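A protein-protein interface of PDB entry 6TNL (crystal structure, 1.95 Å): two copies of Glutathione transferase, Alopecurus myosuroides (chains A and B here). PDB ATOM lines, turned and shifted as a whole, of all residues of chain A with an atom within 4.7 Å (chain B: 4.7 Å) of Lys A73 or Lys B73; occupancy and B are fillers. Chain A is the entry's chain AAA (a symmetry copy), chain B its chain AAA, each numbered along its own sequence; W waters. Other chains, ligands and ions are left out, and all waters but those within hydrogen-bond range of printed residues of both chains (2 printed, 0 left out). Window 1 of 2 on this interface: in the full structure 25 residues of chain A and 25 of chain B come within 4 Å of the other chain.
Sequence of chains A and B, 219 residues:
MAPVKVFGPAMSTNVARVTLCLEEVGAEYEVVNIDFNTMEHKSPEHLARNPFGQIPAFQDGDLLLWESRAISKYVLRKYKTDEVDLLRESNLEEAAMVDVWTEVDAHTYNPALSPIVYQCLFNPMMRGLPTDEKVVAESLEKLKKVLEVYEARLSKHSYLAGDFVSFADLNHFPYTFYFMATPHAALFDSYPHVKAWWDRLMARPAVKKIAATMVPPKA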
ATOM      1  N   ARG A  69      -8.896  35.454  28.837  1.00  0.00           N
ATOM      2  CA  ARG A  69      -8.517  34.033  28.700  1.00  0.00           C
ATOM      3  C   ARG A  69      -6.976  33.902  28.703  1.00  0.00           C
ATOM      4  O   ARG A  69      -6.510  32.947  29.284  1.00  0.00           O
ATOM      5  CB  ARG A  69      -9.122  33.430  27.430  1.00  0.00           C
ATOM      6  CG  ARG A  69     -10.513  32.858  27.658  1.00  0.00           C
ATOM      7  CD  ARG A  69     -11.145  32.170  26.452  1.00  0.00           C
ATOM      8  NE  ARG A  69     -12.087  33.086  25.813  1.00  0.00           N
ATOM      9  CZ  ARG A  69     -13.347  33.306  26.186  1.00  0.00           C
ATOM     10  NH1 ARG A  69     -13.878  32.604  27.164  1.00  0.00           N
ATOM     11  NH2 ARG A  69     -14.126  34.119  25.505  1.00  0.00           N
ATOM     12  N   ALA A  70      -6.259  34.781  28.033  1.00  0.00           N
ATOM     13  CA  ALA A  70      -4.776  34.707  28.003  1.00  0.00           C
ATOM     14  C   ALA A  70      -4.246  34.992  29.421  1.00  0.00           C
ATOM     15  O   ALA A  70      -3.293  34.250  29.904  1.00  0.00           O
ATOM     16  CB  ALA A  70      -4.210  35.643  26.977  1.00  0.00           C
ATOM     17  N   ILE A  71      -4.798  36.006  30.093  1.00  0.00           N
ATOM     18  CA  ILE A  71      -4.407  36.314  31.494  1.00  0.00           C
ATOM     19  C   ILE A  71      -4.621  35.060  32.350  1.00  0.00           C
ATOM     20  O   ILE A  71      -3.700  34.708  33.117  1.00  0.00           O
ATOM     21  CB  ILE A  71      -5.202  37.504  32.064  1.00  0.00           C
ATOM     22  CG1 ILE A  71      -4.894  38.778  31.292  1.00  0.00           C
ATOM     23  CG2 ILE A  71      -4.907  37.687  33.553  1.00  0.00           C
ATOM     24  CD1 ILE A  71      -5.813  39.909  31.608  1.00  0.00           C
ATOM     25  N   SER A  72      -5.815  34.465  32.277  1.00  0.00           N
ATOM     26  CA  SER A  72      -6.216  33.284  33.068  1.00  0.00           C
ATOM     27  C   SER A  72      -5.218  32.137  32.867  1.00  0.00           C
ATOM     28  O   SER A  72      -4.804  31.504  33.874  1.00  0.00           O
ATOM     29  CB  SER A  72      -7.659  32.851  32.759  1.00  0.00           C
ATOM     30  OG  SER A  72      -8.576  33.855  33.190  1.00  0.00           O
ATOM     31  N   LYS A  73      -4.893  31.816  31.632  1.00  0.00           N
ATOM     32  CA  LYS A  73      -3.975  30.685  31.340  1.00  0.00           C
ATOM     33  C   LYS A  73      -2.581  31.002  31.877  1.00  0.00           C
ATOM     34  O   LYS A  73      -1.948  30.081  32.408  1.00  0.00           O
ATOM     35  CB  LYS A  73      -4.018  30.318  29.866  1.00  0.00           C
ATOM     36  CG  LYS A  73      -5.331  29.664  29.483  1.00  0.00           C
ATOM     37  CD  LYS A  73      -5.349  29.257  28.038  1.00  0.00           C
ATOM     38  CE  LYS A  73      -6.091  27.963  27.784  1.00  0.00           C
ATOM     39  NZ  LYS A  73      -5.685  27.428  26.441  1.00  0.00           N
ATOM     40  N   TYR A  74      -2.145  32.251  31.802  1.00  0.00           N
ATOM     41  CA  TYR A  74      -0.822  32.638  32.347  1.00  0.00           C
ATOM     42  C   TYR A  74      -0.815  32.386  33.870  1.00  0.00           C
ATOM     43  O   TYR A  74       0.160  31.760  34.394  1.00  0.00           O
ATOM     44  CB  TYR A  74      -0.493  34.081  32.010  1.00  0.00           C
ATOM     45  CG  TYR A  74       0.707  34.611  32.736  1.00  0.00           C
ATOM     46  CD1 TYR A  74       1.976  34.455  32.220  1.00  0.00           C
ATOM     47  CD2 TYR A  74       0.577  35.263  33.946  1.00  0.00           C
ATOM     48  CE1 TYR A  74       3.082  34.993  32.855  1.00  0.00           C
ATOM     49  CE2 TYR A  74       1.673  35.764  34.624  1.00  0.00           C
ATOM     50  CZ  TYR A  74       2.932  35.640  34.073  1.00  0.00           C
ATOM     51  OH  TYR A  74       4.009  36.167  34.727  1.00  0.00           O
ATOM     52  N   VAL A  75      -1.885  32.785  34.528  1.00  0.00           N
ATOM     53  CA  VAL A  75      -2.087  32.525  35.983  1.00  0.00           C
ATOM     54  C   VAL A  75      -2.069  31.017  36.279  1.00  0.00           C
ATOM     55  O   VAL A  75      -1.301  30.585  37.176  1.00  0.00           O
ATOM     56  CB  VAL A  75      -3.369  33.187  36.501  1.00  0.00           C
ATOM     57  CG1 VAL A  75      -3.704  32.658  37.911  1.00  0.00           C
ATOM     58  CG2 VAL A  75      -3.243  34.700  36.491  1.00  0.00           C
ATOM     59  N   LEU A  76      -2.815  30.224  35.536  1.00  0.00           N
ATOM     60  CA  LEU A  76      -2.912  28.780  35.801  1.00  0.00           C
ATOM     61  C   LEU A  76      -1.584  28.086  35.520  1.00  0.00           C
ATOM     62  O   LEU A  76      -1.303  27.109  36.186  1.00  0.00           O
ATOM     63  CB  LEU A  76      -4.030  28.174  34.968  1.00  0.00           C
ATOM     64  CG  LEU A  76      -5.452  28.645  35.308  1.00  0.00           C
ATOM     65  CD1 LEU A  76      -6.462  27.812  34.533  1.00  0.00           C
ATOM     66  CD2 LEU A  76      -5.728  28.567  36.806  1.00  0.00           C
ATOM     67  N   ARG A  77      -0.789  28.550  34.566  1.00  0.00           N
ATOM     68  CA  ARG A  77       0.539  27.941  34.290  1.00  0.00           C
ATOM     69  C   ARG A  77       1.559  28.422  35.307  1.00  0.00           C
ATOM     70  O   ARG A  77       2.336  27.615  35.766  1.00  0.00           O
ATOM     71  CB  ARG A  77       1.093  28.336  32.919  1.00  0.00           C
ATOM     72  CG  ARG A  77       0.351  27.699  31.762  1.00  0.00           C
ATOM     73  CD  ARG A  77       1.011  28.103  30.453  1.00  0.00           C
ATOM     74  NE  ARG A  77       0.125  27.627  29.397  1.00  0.00           N
ATOM     75  CZ  ARG A  77      -0.501  28.366  28.478  1.00  0.00           C
ATOM     76  NH1 ARG A  77      -0.273  29.673  28.365  1.00  0.00           N
ATOM     77  NH2 ARG A  77      -1.293  27.730  27.635  1.00  0.00           N
ATOM     78  N   LEU A  87      -5.081  23.146  33.704  1.00  0.00           N
ATOM     79  CA  LEU A  87      -5.022  23.030  32.217  1.00  0.00           C
ATOM     80  C   LEU A  87      -4.675  21.600  31.797  1.00  0.00           C
ATOM     81  O   LEU A  87      -4.967  21.243  30.663  1.00  0.00           O
ATOM     82  CB  LEU A  87      -4.021  24.044  31.690  1.00  0.00           C
ATOM     83  CG  LEU A  87      -4.420  25.510  31.910  1.00  0.00           C
ATOM     84  CD1 LEU A  87      -3.274  26.439  31.545  1.00  0.00           C
ATOM     85  CD2 LEU A  87      -5.698  25.903  31.146  1.00  0.00           C
ATOM     86  N   ASP A  99      -9.689  22.110  26.571  1.00  0.00           N
ATOM     87  CA  ASP A  99      -9.791  23.067  25.433  1.00  0.00           C
ATOM     88  C   ASP A  99     -11.190  22.969  24.810  1.00  0.00           C
ATOM     89  O   ASP A  99     -11.799  24.025  24.556  1.00  0.00           O
ATOM     90  CB  ASP A  99      -8.699  22.794  24.393  1.00  0.00           C
ATOM     91  CG  ASP A  99      -7.304  23.197  24.812  1.00  0.00           C
ATOM     92  OD1 ASP A  99      -7.185  23.894  25.837  1.00  0.00           O
ATOM     93  OD2 ASP A  99      -6.366  22.783  24.126  1.00  0.00           O
ATOM     94  N   PHE A 167      -9.989  24.340  34.087  1.00  0.00           N
ATOM     95  CA  PHE A 167     -10.331  25.657  33.512  1.00  0.00           C
ATOM     96  C   PHE A 167     -11.694  25.576  32.832  1.00  0.00           C
ATOM     97  O   PHE A 167     -12.381  26.594  32.809  1.00  0.00           O
ATOM     98  CB  PHE A 167      -9.197  26.087  32.576  1.00  0.00           C
ATOM     99  CG  PHE A 167      -9.298  27.458  31.958  1.00  0.00           C
ATOM    100  CD1 PHE A 167      -9.597  28.558  32.742  1.00  0.00           C
ATOM    101  CD2 PHE A 167      -8.967  27.641  30.639  1.00  0.00           C
ATOM    102  CE1 PHE A 167      -9.589  29.831  32.199  1.00  0.00           C
ATOM    103  CE2 PHE A 167      -8.940  28.912  30.081  1.00  0.00           C
ATOM    104  CZ  PHE A 167      -9.330  30.000  30.857  1.00  0.00           C
ATOM    105  N   ARG B  69     -10.304  25.377  17.303  1.00  0.00           N
ATOM    106  CA  ARG B  69      -9.150  25.807  18.118  1.00  0.00           C
ATOM    107  C   ARG B  69      -8.675  24.635  19.008  1.00  0.00           C
ATOM    108  O   ARG B  69      -7.479  24.516  19.161  1.00  0.00           O
ATOM    109  CB  ARG B  69      -9.510  27.033  18.961  1.00  0.00           C
ATOM    110  CG  ARG B  69      -9.259  28.342  18.229  1.00  0.00           C
ATOM    111  CD  ARG B  69      -9.521  29.608  19.039  1.00  0.00           C
ATOM    112  NE  ARG B  69     -10.831  30.147  18.682  1.00  0.00           N
ATOM    113  CZ  ARG B  69     -11.104  30.918  17.630  1.00  0.00           C
ATOM    114  NH1 ARG B  69     -10.133  31.335  16.847  1.00  0.00           N
ATOM    115  NH2 ARG B  69     -12.316  31.392  17.430  1.00  0.00           N
ATOM    116  N   ALA B  70      -9.574  23.874  19.597  1.00  0.00           N
ATOM    117  CA  ALA B  70      -9.176  22.733  20.460  1.00  0.00           C
ATOM    118  C   ALA B  70      -8.499  21.668  19.575  1.00  0.00           C
ATOM    119  O   ALA B  70      -7.413  21.091  19.995  1.00  0.00           O
ATOM    120  CB  ALA B  70     -10.354  22.191  21.215  1.00  0.00           C
ATOM    121  N   ILE B  71      -9.076  21.383  18.404  1.00  0.00           N
ATOM    122  CA  ILE B  71      -8.461  20.424  17.449  1.00  0.00           C
ATOM    123  C   ILE B  71      -7.038  20.897  17.127  1.00  0.00           C
ATOM    124  O   ILE B  71      -6.114  20.057  17.177  1.00  0.00           O
ATOM    125  CB  ILE B  71      -9.291  20.285  16.159  1.00  0.00           C
ATOM    126  CG1 ILE B  71     -10.661  19.698  16.461  1.00  0.00           C
ATOM    127  CG2 ILE B  71      -8.551  19.433  15.128  1.00  0.00           C
ATOM    128  CD1 ILE B  71     -11.615  19.777  15.316  1.00  0.00           C
ATOM    129  N   SER B  72      -6.887  22.166  16.738  1.00  0.00           N
ATOM    130  CA  SER B  72      -5.604  22.777  16.338  1.00  0.00           C
ATOM    131  C   SER B  72      -4.555  22.602  17.444  1.00  0.00           C
ATOM    132  O   SER B  72      -3.398  22.219  17.133  1.00  0.00           O
ATOM    133  CB  SER B  72      -5.771  24.251  15.934  1.00  0.00           C
ATOM    134  OG  SER B  72      -6.559  24.349  14.748  1.00  0.00           O
ATOM    135  N   LYS B  73      -4.898  22.934  18.672  1.00  0.00           N
ATOM    136  CA  LYS B  73      -3.932  22.848  19.798  1.00  0.00           C
ATOM    137  C   LYS B  73      -3.557  21.388  20.042  1.00  0.00           C
ATOM    138  O   LYS B  73      -2.377  21.136  20.315  1.00  0.00           O
ATOM    139  CB  LYS B  73      -4.457  23.581  21.020  1.00  0.00           C
ATOM    140  CG  LYS B  73      -4.457  25.084  20.822  1.00  0.00           C
ATOM    141  CD  LYS B  73      -4.929  25.807  22.050  1.00  0.00           C
ATOM    142  CE  LYS B  73      -4.209  27.116  22.294  1.00  0.00           C
ATOM    143  NZ  LYS B  73      -4.420  27.526  23.724  1.00  0.00           N
ATOM    144  N   TYR B  74      -4.494  20.462  19.896  1.00  0.00           N
ATOM    145  CA  TYR B  74      -4.189  19.023  20.072  1.00  0.00           C
ATOM    146  C   TYR B  74      -3.150  18.599  19.012  1.00  0.00           C
ATOM    147  O   TYR B  74      -2.127  17.934  19.371  1.00  0.00           O
ATOM    148  CB  TYR B  74      -5.451  18.183  19.996  1.00  0.00           C
ATOM    149  CG  TYR B  74      -5.190  16.709  19.916  1.00  0.00           C
ATOM    150  CD1 TYR B  74      -5.044  15.950  21.059  1.00  0.00           C
ATOM    151  CD2 TYR B  74      -5.079  16.070  18.698  1.00  0.00           C
ATOM    152  CE1 TYR B  74      -4.861  14.579  20.993  1.00  0.00           C
ATOM    153  CE2 TYR B  74      -4.846  14.710  18.609  1.00  0.00           C
ATOM    154  CZ  TYR B  74      -4.747  13.956  19.760  1.00  0.00           C
ATOM    155  OH  TYR B  74      -4.553  12.607  19.669  1.00  0.00           O
ATOM    156  N   VAL B  75      -3.365  19.031  17.784  1.00  0.00           N
ATOM    157  CA  VAL B  75      -2.407  18.802  16.665  1.00  0.00           C
ATOM    158  C   VAL B  75      -1.032  19.409  16.985  1.00  0.00           C
ATOM    159  O   VAL B  75      -0.011  18.686  16.880  1.00  0.00           O
ATOM    160  CB  VAL B  75      -2.960  19.326  15.334  1.00  0.00           C
ATOM    161  CG1 VAL B  75      -1.843  19.350  14.271  1.00  0.00           C
ATOM    162  CG2 VAL B  75      -4.148  18.499  14.875  1.00  0.00           C
ATOM    163  N   LEU B  76      -0.984  20.653  17.419  1.00  0.00           N
ATOM    164  CA  LEU B  76       0.295  21.334  17.678  1.00  0.00           C
ATOM    165  C   LEU B  76       1.015  20.704  18.865  1.00  0.00           C
ATOM    166  O   LEU B  76       2.231  20.714  18.861  1.00  0.00           O
ATOM    167  CB  LEU B  76       0.057  22.816  17.910  1.00  0.00           C
ATOM    168  CG  LEU B  76      -0.475  23.608  16.705  1.00  0.00           C
ATOM    169  CD1 LEU B  76      -0.475  25.094  17.033  1.00  0.00           C
ATOM    170  CD2 LEU B  76       0.343  23.336  15.447  1.00  0.00           C
ATOM    171  N   ARG B  77       0.312  20.181  19.859  1.00  0.00           N
ATOM    172  CA  ARG B  77       0.966  19.510  21.012  1.00  0.00           C
ATOM    173  C   ARG B  77       1.382  18.100  20.631  1.00  0.00           C
ATOM    174  O   ARG B  77       2.467  17.703  20.996  1.00  0.00           O
ATOM    175  CB  ARG B  77       0.030  19.361  22.214  1.00  0.00           C
ATOM    176  CG  ARG B  77      -0.272  20.673  22.909  1.00  0.00           C
ATOM    177  CD  ARG B  77      -1.155  20.414  24.119  1.00  0.00           C
ATOM    178  NE  ARG B  77      -1.566  21.726  24.602  1.00  0.00           N
ATOM    179  CZ  ARG B  77      -2.812  22.198  24.692  1.00  0.00           C
ATOM    180  NH1 ARG B  77      -3.866  21.425  24.439  1.00  0.00           N
ATOM    181  NH2 ARG B  77      -2.955  23.438  25.122  1.00  0.00           N
ATOM    182  N   LEU B  87       3.139  26.532  20.073  1.00  0.00           N
ATOM    183  CA  LEU B  87       2.431  27.068  21.272  1.00  0.00           C
ATOM    184  C   LEU B  87       3.428  27.629  22.288  1.00  0.00           C
ATOM    185  O   LEU B  87       3.022  28.437  23.112  1.00  0.00           O
ATOM    186  CB  LEU B  87       1.569  25.963  21.862  1.00  0.00           C
ATOM    187  CG  LEU B  87       0.420  25.498  20.956  1.00  0.00           C
ATOM    188  CD1 LEU B  87      -0.250  24.261  21.531  1.00  0.00           C
ATOM    189  CD2 LEU B  87      -0.621  26.603  20.694  1.00  0.00           C
ATOM    190  N   ASP B  99      -1.048  33.251  23.314  1.00  0.00           N
ATOM    191  CA  ASP B  99      -2.463  33.274  23.780  1.00  0.00           C
ATOM    192  C   ASP B  99      -3.061  34.664  23.520  1.00  0.00           C
ATOM    193  O   ASP B  99      -4.192  34.732  23.003  1.00  0.00           O
ATOM    194  CB  ASP B  99      -2.553  32.900  25.264  1.00  0.00           C
ATOM    195  CG  ASP B  99      -2.312  31.440  25.569  1.00  0.00           C
ATOM    196  OD1 ASP B  99      -2.279  30.645  24.611  1.00  0.00           O
ATOM    197  OD2 ASP B  99      -2.132  31.132  26.749  1.00  0.00           O
ATOM    198  N   PHE B 167       1.217  29.752  16.668  1.00  0.00           N
ATOM    199  CA  PHE B 167      -0.236  29.594  16.449  1.00  0.00           C
ATOM    200  C   PHE B 167      -0.870  30.967  16.244  1.00  0.00           C
ATOM    201  O   PHE B 167      -1.863  31.034  15.524  1.00  0.00           O
ATOM    202  CB  PHE B 167      -0.822  28.811  17.627  1.00  0.00           C
ATOM    203  CG  PHE B 167      -2.283  28.449  17.553  1.00  0.00           C
ATOM    204  CD1 PHE B 167      -2.807  27.881  16.406  1.00  0.00           C
ATOM    205  CD2 PHE B 167      -3.074  28.563  18.668  1.00  0.00           C
ATOM    206  CE1 PHE B 167      -4.122  27.453  16.370  1.00  0.00           C
ATOM    207  CE2 PHE B 167      -4.391  28.126  18.655  1.00  0.00           C
ATOM    208  CZ  PHE B 167      -4.931  27.639  17.468  1.00  0.00           C
HETATM  209  O   HOH W   1      -1.322  32.892  28.725  1.00  0.00           O
HETATM  210  O   HOH W   2      -6.499  20.586  22.450  1.00  0.00           O
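Ala A70 touches Asp B99, and with the chains exchanged Asp A99 touches Ala B70. Lys B73 touches its own counterpart, Lys A73. Lys A73 touches Asp B99, and with the chains exchanged Asp A99 touches Lys B73. Arg A77 touches Asp B99, and with the chains exchanged Asp A99 touches Arg B77. Positions printed for both chains: 69, 70, 71, 72, 73, 74, 75, 76, 77, 87, 99 and 167.
Water W2 lies within hydrogen-bond range of the backbone carbonyl oxygen (O) of Ala B70 (2.7 Å), the side-chain carboxylate (OD2) of Asp A99 (2.8 Å), the backbone NH (N) of Tyr B74 (3.2 Å) and the guanidinium group (NH1) of Arg B77 (3.4 Å). Water W1 lies within hydrogen-bond range of the backbone carbonyl oxygen of Ala A70, the side-chain carboxylate of Asp B99, the backbone NH of Tyr A74 and the guanidinium group of Arg A77.
NZ of Lys B73 is in salt-bridge range of OD1 of Asp B99. The side-chain amino group (NZ) of Lys A73 lies within salt-bridge range of the side-chain carboxylate (OD1) of Asp A99, 3.9 Å away.
Among the printed residues, merely in contact across the chains: Asp A99 with Ala B70 (3.6 Å), Ala A70 with Asp B99 (3.6 Å), Asp A99 with Lys B73 (3.7 Å) and Lys A73 with Asp B99 (3.7 Å).
Of the printed residues of chain B, Ala A70 touches Asp B99 (3.6 Å). Ile A71 touches none of the printed residues of chain B. Lys A73 touches just these residues of chain B: Lys B73 and Asp B99. Of the printed residues of chain B, Asp A99 touches Ala B70 (3.6 Å), Lys B73 (3.7 Å) and Arg B77 (2.9 Å). Lys B73 touches two residues of chain A. The nearest printed residue of chain A that does not touch Ala B70 is Lys A73 (8.4 Å).
The guanidinium group of Arg A77 lies within salt-bridge range of the side-chain carboxylate of Asp B99, at 2.9 Å. NH1 of Arg B77 lies within salt-bridge range of OD2 of Asp A99 (2.9 Å). NZ of Lys B73 sits close to NZ of Lys A73.
Along chain A the printed residues that touch a printed residue of chain B span positions 70 to 99.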
